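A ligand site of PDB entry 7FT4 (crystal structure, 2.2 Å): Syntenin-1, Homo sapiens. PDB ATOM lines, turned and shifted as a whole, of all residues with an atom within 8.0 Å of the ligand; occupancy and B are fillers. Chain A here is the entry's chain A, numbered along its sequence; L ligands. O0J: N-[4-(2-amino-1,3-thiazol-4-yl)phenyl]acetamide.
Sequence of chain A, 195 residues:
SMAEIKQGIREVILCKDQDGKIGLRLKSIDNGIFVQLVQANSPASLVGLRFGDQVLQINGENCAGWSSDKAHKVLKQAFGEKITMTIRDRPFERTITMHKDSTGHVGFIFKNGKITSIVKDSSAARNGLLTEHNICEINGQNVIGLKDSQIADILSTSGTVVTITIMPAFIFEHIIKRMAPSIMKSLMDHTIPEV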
ATOM      1  N   GLY A  20     -12.943  14.407  -7.237  1.00  0.00           N
ATOM      2  CA  GLY A  20     -12.846  13.909  -5.881  1.00  0.00           C
ATOM      3  C   GLY A  20     -13.100  12.412  -5.788  1.00  0.00           C
ATOM      4  O   GLY A  20     -13.544  11.923  -4.753  1.00  0.00           O
ATOM      5  N   LYS A  21     -12.774  11.696  -6.881  1.00  0.00           N
ATOM      6  CA  LYS A  21     -13.015  10.273  -7.043  1.00  0.00           C
ATOM      7  C   LYS A  21     -11.714   9.482  -7.066  1.00  0.00           C
ATOM      8  O   LYS A  21     -10.721   9.926  -7.623  1.00  0.00           O
ATOM      9  CB  LYS A  21     -13.734   9.997  -8.370  1.00  0.00           C
ATOM     10  CG  LYS A  21     -15.245   9.858  -8.256  1.00  0.00           C
ATOM     11  CD  LYS A  21     -15.850   9.110  -9.431  1.00  0.00           C
ATOM     12  CE  LYS A  21     -16.141  10.024 -10.590  1.00  0.00           C
ATOM     13  NZ  LYS A  21     -17.240  10.961 -10.252  1.00  0.00           N
ATOM     14  N   ILE A  22     -11.749   8.269  -6.517  1.00  0.00           N
ATOM     15  CA  ILE A  22     -10.617   7.385  -6.698  1.00  0.00           C
ATOM     16  C   ILE A  22     -10.965   6.227  -7.634  1.00  0.00           C
ATOM     17  O   ILE A  22     -10.050   5.611  -8.191  1.00  0.00           O
ATOM     18  CB  ILE A  22     -10.074   6.947  -5.338  1.00  0.00           C
ATOM     19  CG1 ILE A  22     -11.143   6.301  -4.465  1.00  0.00           C
ATOM     20  CG2 ILE A  22      -9.477   8.143  -4.622  1.00  0.00           C
ATOM     21  CD1 ILE A  22     -10.567   5.646  -3.263  1.00  0.00           C
ATOM     22  N   GLY A  23     -12.261   5.996  -7.854  1.00  0.00           N
ATOM     23  CA  GLY A  23     -12.738   5.026  -8.842  1.00  0.00           C
ATOM     24  C   GLY A  23     -12.739   3.601  -8.296  1.00  0.00           C
ATOM     25  O   GLY A  23     -12.445   2.627  -8.998  1.00  0.00           O
ATOM     26  N   LEU A  24     -13.136   3.502  -7.021  1.00  0.00           N
ATOM     27  CA  LEU A  24     -12.914   2.307  -6.245  1.00  0.00           C
ATOM     28  C   LEU A  24     -14.120   2.043  -5.348  1.00  0.00           C
ATOM     29  O   LEU A  24     -14.727   2.944  -4.776  1.00  0.00           O
ATOM     30  CB  LEU A  24     -11.620   2.573  -5.473  1.00  0.00           C
ATOM     31  CG  LEU A  24     -11.045   1.444  -4.642  1.00  0.00           C
ATOM     32  CD1 LEU A  24     -10.650   0.246  -5.478  1.00  0.00           C
ATOM     33  CD2 LEU A  24      -9.829   1.953  -3.905  1.00  0.00           C
ATOM     34  N   ARG A  25     -14.448   0.753  -5.254  1.00  0.00           N
ATOM     35  CA  ARG A  25     -15.548   0.229  -4.469  1.00  0.00           C
ATOM     36  C   ARG A  25     -15.029  -0.967  -3.676  1.00  0.00           C
ATOM     37  O   ARG A  25     -14.516  -1.922  -4.288  1.00  0.00           O
ATOM     38  CB  ARG A  25     -16.649  -0.166  -5.476  1.00  0.00           C
ATOM     39  CG  ARG A  25     -17.709  -1.143  -4.988  1.00  0.00           C
ATOM     40  CD  ARG A  25     -18.828  -0.596  -4.130  1.00  0.00           C
ATOM     41  NE  ARG A  25     -20.104  -1.299  -4.302  1.00  0.00           N
ATOM     42  CZ  ARG A  25     -21.057  -1.374  -3.371  1.00  0.00           C
ATOM     43  NH1 ARG A  25     -22.133  -2.096  -3.602  1.00  0.00           N
ATOM     44  NH2 ARG A  25     -20.914  -0.749  -2.208  1.00  0.00           N
ATOM     45  N   LEU A  26     -15.171  -0.930  -2.345  1.00  0.00           N
ATOM     46  CA  LEU A  26     -14.655  -1.943  -1.434  1.00  0.00           C
ATOM     47  C   LEU A  26     -15.790  -2.795  -0.852  1.00  0.00           C
ATOM     48  O   LEU A  26     -16.929  -2.367  -0.872  1.00  0.00           O
ATOM     49  CB  LEU A  26     -13.932  -1.204  -0.310  1.00  0.00           C
ATOM     50  CG  LEU A  26     -12.805  -0.263  -0.701  1.00  0.00           C
ATOM     51  CD1 LEU A  26     -12.433   0.626   0.486  1.00  0.00           C
ATOM     52  CD2 LEU A  26     -11.594  -1.020  -1.212  1.00  0.00           C
ATOM     53  N   GLN A  36     -14.086  -4.703  -4.482  1.00  0.00           N
ATOM     54  CA  GLN A  36     -15.239  -5.206  -5.208  1.00  0.00           C
ATOM     55  C   GLN A  36     -15.216  -4.671  -6.644  1.00  0.00           C
ATOM     56  O   GLN A  36     -15.599  -5.376  -7.572  1.00  0.00           O
ATOM     57  CB  GLN A  36     -16.496  -4.804  -4.427  1.00  0.00           C
ATOM     58  CG  GLN A  36     -17.808  -5.208  -5.107  1.00  0.00           C
ATOM     59  CD  GLN A  36     -19.065  -4.753  -4.391  1.00  0.00           C
ATOM     60  OE1 GLN A  36     -19.372  -3.566  -4.307  1.00  0.00           O
ATOM     61  NE2 GLN A  36     -19.835  -5.712  -3.907  1.00  0.00           N
ATOM     62  N   LEU A  37     -14.761  -3.427  -6.836  1.00  0.00           N
ATOM     63  CA  LEU A  37     -14.963  -2.781  -8.122  1.00  0.00           C
ATOM     64  C   LEU A  37     -13.901  -1.716  -8.384  1.00  0.00           C
ATOM     65  O   LEU A  37     -13.691  -0.815  -7.581  1.00  0.00           O
ATOM     66  CB  LEU A  37     -16.363  -2.160  -8.074  1.00  0.00           C
ATOM     67  CG  LEU A  37     -17.160  -2.275  -9.358  1.00  0.00           C
ATOM     68  CD1 LEU A  37     -18.556  -1.702  -9.160  1.00  0.00           C
ATOM     69  CD2 LEU A  37     -16.438  -1.566 -10.493  1.00  0.00           C
ATOM     70  N   VAL A  38     -13.234  -1.807  -9.535  1.00  0.00           N
ATOM     71  CA  VAL A  38     -12.357  -0.733  -9.943  1.00  0.00           C
ATOM     72  C   VAL A  38     -12.758  -0.197 -11.310  1.00  0.00           C
ATOM     73  O   VAL A  38     -12.741  -0.922 -12.314  1.00  0.00           O
ATOM     74  CB  VAL A  38     -10.884  -1.120  -9.883  1.00  0.00           C
ATOM     75  CG1 VAL A  38     -10.001  -0.200 -10.713  1.00  0.00           C
ATOM     76  CG2 VAL A  38     -10.396  -1.143  -8.445  1.00  0.00           C
ATOM     77  N   GLN A  39     -13.011   1.121 -11.310  1.00  0.00           N
ATOM     78  CA  GLN A  39     -13.474   1.925 -12.421  1.00  0.00           C
ATOM     79  C   GLN A  39     -12.327   2.136 -13.413  1.00  0.00           C
ATOM     80  O   GLN A  39     -11.202   2.450 -13.005  1.00  0.00           O
ATOM     81  CB  GLN A  39     -14.020   3.208 -11.800  1.00  0.00           C
ATOM     82  CG  GLN A  39     -14.803   4.111 -12.754  1.00  0.00           C
ATOM     83  CD  GLN A  39     -15.571   5.223 -12.051  1.00  0.00           C
ATOM     84  OE1 GLN A  39     -15.074   5.903 -11.159  1.00  0.00           O
ATOM     85  NE2 GLN A  39     -16.815   5.423 -12.464  1.00  0.00           N
ATOM     86  N   SER A  68     -18.002  -1.892   4.813  1.00  0.00           N
ATOM     87  CA  SER A  68     -17.865  -1.283   3.497  1.00  0.00           C
ATOM     88  C   SER A  68     -18.150   0.211   3.592  1.00  0.00           C
ATOM     89  O   SER A  68     -17.399   1.026   3.060  1.00  0.00           O
ATOM     90  CB  SER A  68     -18.777  -1.965   2.517  1.00  0.00           C
ATOM     91  OG  SER A  68     -18.742  -3.379   2.689  1.00  0.00           O
ATOM     92  N   ASP A  69     -19.220   0.573   4.299  1.00  0.00           N
ATOM     93  CA  ASP A  69     -19.665   1.967   4.323  1.00  0.00           C
ATOM     94  C   ASP A  69     -18.596   2.819   4.999  1.00  0.00           C
ATOM     95  O   ASP A  69     -18.259   3.879   4.483  1.00  0.00           O
ATOM     96  CB  ASP A  69     -21.055   2.129   4.929  1.00  0.00           C
ATOM     97  CG  ASP A  69     -22.157   1.758   3.956  1.00  0.00           C
ATOM     98  OD1 ASP A  69     -22.013   2.078   2.771  1.00  0.00           O
ATOM     99  OD2 ASP A  69     -23.152   1.168   4.387  1.00  0.00           O
ATOM    100  N   ALA A  71     -15.371   2.240   5.189  1.00  0.00           N
ATOM    101  CA  ALA A  71     -14.168   2.382   4.392  1.00  0.00           C
ATOM    102  C   ALA A  71     -14.390   3.466   3.355  1.00  0.00           C
ATOM    103  O   ALA A  71     -13.517   4.312   3.177  1.00  0.00           O
ATOM    104  CB  ALA A  71     -13.798   1.078   3.733  1.00  0.00           C
ATOM    105  N   HIS A  72     -15.571   3.460   2.714  1.00  0.00           N
ATOM    106  CA  HIS A  72     -15.976   4.542   1.822  1.00  0.00           C
ATOM    107  C   HIS A  72     -15.954   5.870   2.596  1.00  0.00           C
ATOM    108  O   HIS A  72     -15.337   6.844   2.154  1.00  0.00           O
ATOM    109  CB  HIS A  72     -17.322   4.256   1.161  1.00  0.00           C
ATOM    110  CG  HIS A  72     -17.344   3.033   0.273  1.00  0.00           C
ATOM    111  ND1 HIS A  72     -18.517   2.446  -0.149  1.00  0.00           N
ATOM    112  CD2 HIS A  72     -16.353   2.275  -0.244  1.00  0.00           C
ATOM    113  CE1 HIS A  72     -18.260   1.368  -0.888  1.00  0.00           C
ATOM    114  NE2 HIS A  72     -16.954   1.256  -0.968  1.00  0.00           N
ATOM    115  N   LYS A  73     -16.545   5.888   3.795  1.00  0.00           N
ATOM    116  CA  LYS A  73     -16.567   7.095   4.616  1.00  0.00           C
ATOM    117  C   LYS A  73     -15.166   7.664   4.846  1.00  0.00           C
ATOM    118  O   LYS A  73     -14.997   8.878   4.907  1.00  0.00           O
ATOM    119  CB  LYS A  73     -17.219   6.825   5.970  1.00  0.00           C
ATOM    120  CG  LYS A  73     -17.686   8.094   6.688  1.00  0.00           C
ATOM    121  CD  LYS A  73     -18.750   7.863   7.742  1.00  0.00           C
ATOM    122  CE  LYS A  73     -19.004   9.088   8.593  1.00  0.00           C
ATOM    123  NZ  LYS A  73     -20.056   8.860   9.619  1.00  0.00           N
ATOM    124  N   VAL A  74     -14.175   6.783   5.018  1.00  0.00           N
ATOM    125  CA  VAL A  74     -12.817   7.172   5.368  1.00  0.00           C
ATOM    126  C   VAL A  74     -12.142   7.802   4.154  1.00  0.00           C
ATOM    127  O   VAL A  74     -11.501   8.854   4.236  1.00  0.00           O
ATOM    128  CB  VAL A  74     -12.078   5.937   5.912  1.00  0.00           C
ATOM    129  CG1 VAL A  74     -10.573   6.060   5.841  1.00  0.00           C
ATOM    130  CG2 VAL A  74     -12.535   5.620   7.334  1.00  0.00           C
ATOM    131  N   LEU A  75     -12.317   7.147   3.003  1.00  0.00           N
ATOM    132  CA  LEU A  75     -11.760   7.633   1.748  1.00  0.00           C
ATOM    133  C   LEU A  75     -12.279   9.034   1.420  1.00  0.00           C
ATOM    134  O   LEU A  75     -11.571   9.793   0.744  1.00  0.00           O
ATOM    135  CB  LEU A  75     -12.149   6.653   0.638  1.00  0.00           C
ATOM    136  CG  LEU A  75     -11.388   5.331   0.688  1.00  0.00           C
ATOM    137  CD1 LEU A  75     -12.017   4.300  -0.244  1.00  0.00           C
ATOM    138  CD2 LEU A  75      -9.939   5.581   0.336  1.00  0.00           C
ATOM    139  N   LYS A  76     -13.501   9.353   1.843  1.00  0.00           N
ATOM    140  CA  LYS A  76     -14.118  10.631   1.539  1.00  0.00           C
ATOM    141  C   LYS A  76     -13.473  11.707   2.408  1.00  0.00           C
ATOM    142  O   LYS A  76     -12.844  12.614   1.889  1.00  0.00           O
ATOM    143  CB  LYS A  76     -15.632  10.557   1.765  1.00  0.00           C
ATOM    144  CG  LYS A  76     -16.499  11.446   0.856  1.00  0.00           C
ATOM    145  CD  LYS A  76     -17.179  10.711  -0.280  1.00  0.00           C
ATOM    146  CE  LYS A  76     -18.339  11.483  -0.871  1.00  0.00           C
ATOM    147  NZ  LYS A  76     -18.802  10.891  -2.152  1.00  0.00           N
ATOM    148  N   LYS A 177     -21.680  -9.053  -4.644  1.00  0.00           N
ATOM    149  CA  LYS A 177     -23.060  -8.793  -4.258  1.00  0.00           C
ATOM    150  C   LYS A 177     -23.196  -7.320  -3.877  1.00  0.00           C
ATOM    151  O   LYS A 177     -22.216  -6.698  -3.452  1.00  0.00           O
ATOM    152  CB  LYS A 177     -23.514  -9.720  -3.119  1.00  0.00           C
ATOM    153  CG  LYS A 177     -23.853 -11.143  -3.535  1.00  0.00           C
ATOM    154  CD  LYS A 177     -24.177 -12.088  -2.389  1.00  0.00           C
ATOM    155  CE  LYS A 177     -24.895 -13.332  -2.884  1.00  0.00           C
ATOM    156  NZ  LYS A 177     -25.051 -14.365  -1.834  1.00  0.00           N
ATOM    157  N   ARG A 178     -24.419  -6.795  -4.016  1.00  0.00           N
ATOM    158  CA  ARG A 178     -24.708  -5.365  -3.920  1.00  0.00           C
ATOM    159  C   ARG A 178     -24.227  -4.712  -5.224  1.00  0.00           C
ATOM    160  O   ARG A 178     -23.711  -3.596  -5.221  1.00  0.00           O
ATOM    161  CB  ARG A 178     -24.116  -4.767  -2.625  1.00  0.00           C
ATOM    162  CG  ARG A 178     -24.311  -5.623  -1.366  1.00  0.00           C
ATOM    163  CD  ARG A 178     -25.674  -5.501  -0.709  1.00  0.00           C
ATOM    164  NE  ARG A 178     -26.235  -6.744  -0.190  1.00  0.00           N
ATOM    165  CZ  ARG A 178     -27.422  -7.264  -0.535  1.00  0.00           C
ATOM    166  NH1 ARG A 178     -28.199  -6.620  -1.387  1.00  0.00           N
ATOM    167  NH2 ARG A 178     -27.833  -8.422  -0.051  1.00  0.00           N
ATOM    168  N   MET A 179     -24.447  -5.441  -6.327  1.00  0.00           N
ATOM    169  CA  MET A 179     -24.051  -5.073  -7.682  1.00  0.00           C
ATOM    170  C   MET A 179     -24.729  -5.989  -8.703  1.00  0.00           C
ATOM    171  O   MET A 179     -24.708  -7.208  -8.547  1.00  0.00           O
ATOM    172  CB  MET A 179     -22.547  -5.220  -7.850  1.00  0.00           C
ATOM    173  CG  MET A 179     -21.821  -3.925  -7.765  1.00  0.00           C
ATOM    174  SD  MET A 179     -20.136  -4.309  -7.353  1.00  0.00           S
ATOM    175  CE  MET A 179     -19.625  -5.088  -8.881  1.00  0.00           C
ATOM    176  N   ALA A 180     -25.298  -5.389  -9.762  1.00  0.00           N
ATOM    177  CA  ALA A 180     -25.886  -6.134 -10.871  1.00  0.00           C
ATOM    178  C   ALA A 180     -24.782  -6.714 -11.765  1.00  0.00           C
ATOM    179  O   ALA A 180     -23.672  -6.180 -11.778  1.00  0.00           O
ATOM    180  CB  ALA A 180     -26.819  -5.216 -11.635  1.00  0.00           C
ATOM    181  N   ILE A 183     -23.925  -4.422 -14.878  1.00  0.00           N
ATOM    182  CA  ILE A 183     -23.303  -3.243 -14.310  1.00  0.00           C
ATOM    183  C   ILE A 183     -21.792  -3.474 -14.278  1.00  0.00           C
ATOM    184  O   ILE A 183     -21.020  -2.639 -14.745  1.00  0.00           O
ATOM    185  CB  ILE A 183     -23.889  -2.927 -12.909  1.00  0.00           C
ATOM    186  CG1 ILE A 183     -25.122  -2.031 -13.024  1.00  0.00           C
ATOM    187  CG2 ILE A 183     -22.860  -2.325 -11.971  1.00  0.00           C
ATOM    188  CD1 ILE A 183     -26.116  -2.480 -14.089  1.00  0.00           C
ATOM    189  N   MET A 184     -21.404  -4.640 -13.769  1.00  0.00           N
ATOM    190  CA  MET A 184     -20.016  -5.060 -13.720  1.00  0.00           C
ATOM    191  C   MET A 184     -19.425  -5.101 -15.131  1.00  0.00           C
ATOM    192  O   MET A 184     -18.234  -4.864 -15.292  1.00  0.00           O
ATOM    193  CB  MET A 184     -19.884  -6.444 -13.118  1.00  0.00           C
ATOM    194  CG  MET A 184     -19.839  -6.422 -11.635  1.00  0.00           C
ATOM    195  SD  MET A 184     -19.466  -8.067 -11.001  1.00  0.00           S
ATOM    196  CE  MET A 184     -20.815  -9.057 -11.642  1.00  0.00           C
ATOM    197  N   LEU A 187     -18.957  -0.974 -15.431  1.00  0.00           N
ATOM    198  CA  LEU A 187     -18.153  -0.250 -14.458  1.00  0.00           C
ATOM    199  C   LEU A 187     -16.738  -0.832 -14.300  1.00  0.00           C
ATOM    200  O   LEU A 187     -15.784  -0.065 -14.260  1.00  0.00           O
ATOM    201  CB  LEU A 187     -18.920  -0.294 -13.141  1.00  0.00           C
ATOM    202  CG  LEU A 187     -20.367   0.166 -13.271  1.00  0.00           C
ATOM    203  CD1 LEU A 187     -21.028   0.314 -11.894  1.00  0.00           C
ATOM    204  CD2 LEU A 187     -20.433   1.456 -14.060  1.00  0.00           C
HETATM  205  N1  O0J L   1     -23.181  -0.191  -9.129  1.00  0.00           N
HETATM  206  C4  O0J L   1     -20.665   2.485  -4.041  1.00  0.00           C
HETATM  207  C5  O0J L   1     -20.474   1.911  -5.306  1.00  0.00           C
HETATM  208  C6  O0J L   1     -19.233   1.975  -5.923  1.00  0.00           C
HETATM  209  C7  O0J L   1     -18.205   2.636  -5.290  1.00  0.00           C
HETATM  210  C8  O0J L   1     -21.545   1.141  -6.046  1.00  0.00           C
HETATM  211  C10 O0J L   1     -22.750   0.184  -7.819  1.00  0.00           C
HETATM  212  N   O0J L   1     -17.152   3.872  -3.522  1.00  0.00           N
HETATM  213  C   O0J L   1     -15.714   5.468  -2.195  1.00  0.00           C
HETATM  214  O   O0J L   1     -18.072   5.481  -2.047  1.00  0.00           O
HETATM  215  C1  O0J L   1     -17.111   4.974  -2.553  1.00  0.00           C
HETATM  216  C2  O0J L   1     -18.365   3.216  -4.044  1.00  0.00           C
HETATM  217  C3  O0J L   1     -19.612   3.164  -3.414  1.00  0.00           C
HETATM  218  C9  O0J L   1     -22.573   0.452  -5.361  1.00  0.00           C
HETATM  219  N2  O0J L   1     -21.657   0.979  -7.517  1.00  0.00           N
HETATM  220  S   O0J L   1     -23.492  -0.298  -6.440  1.00  0.00           S
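The backbone carbonyl oxygen (O) of Leu 24 lies within hydrogen-bond range of a nitrogen (N) of the ligand (2.9 Å).
A sulfur (S) of the ligand lies close to the guanidinium group of Arg 25 (3.6 Å).
A sulfur (S) of the ligand lies close to the backbone carbonyl oxygen (O) of Arg 178.
His 72 touches the ligand.
Ile 183 touches the ligand.
Leu 187 touches the ligand (CD1 to N1, 3.5 Å).
Hydrophobic or aromatic side chains within 4 Å of the ligand: His 72, Ile 183 and Leu 187.
The nearest printed residue that does not touch the ligand is Met 179 (4.2 Å).
NH1 of Arg 25 lies within hydrogen-bond range of O of Arg 178, at 2.7 Å.
O of Leu 37 sits at hydrogen-bond distance from N of Arg 25 (2.9 Å).
The backbone carbonyl oxygen (O) of Arg 25 is in hydrogen-bond range of the backbone NH (N) of Gln 36, 2.8 Å away.
A ring nitrogen (NE2) of His 72 is in hydrogen-bond range of the backbone NH of Leu 26.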
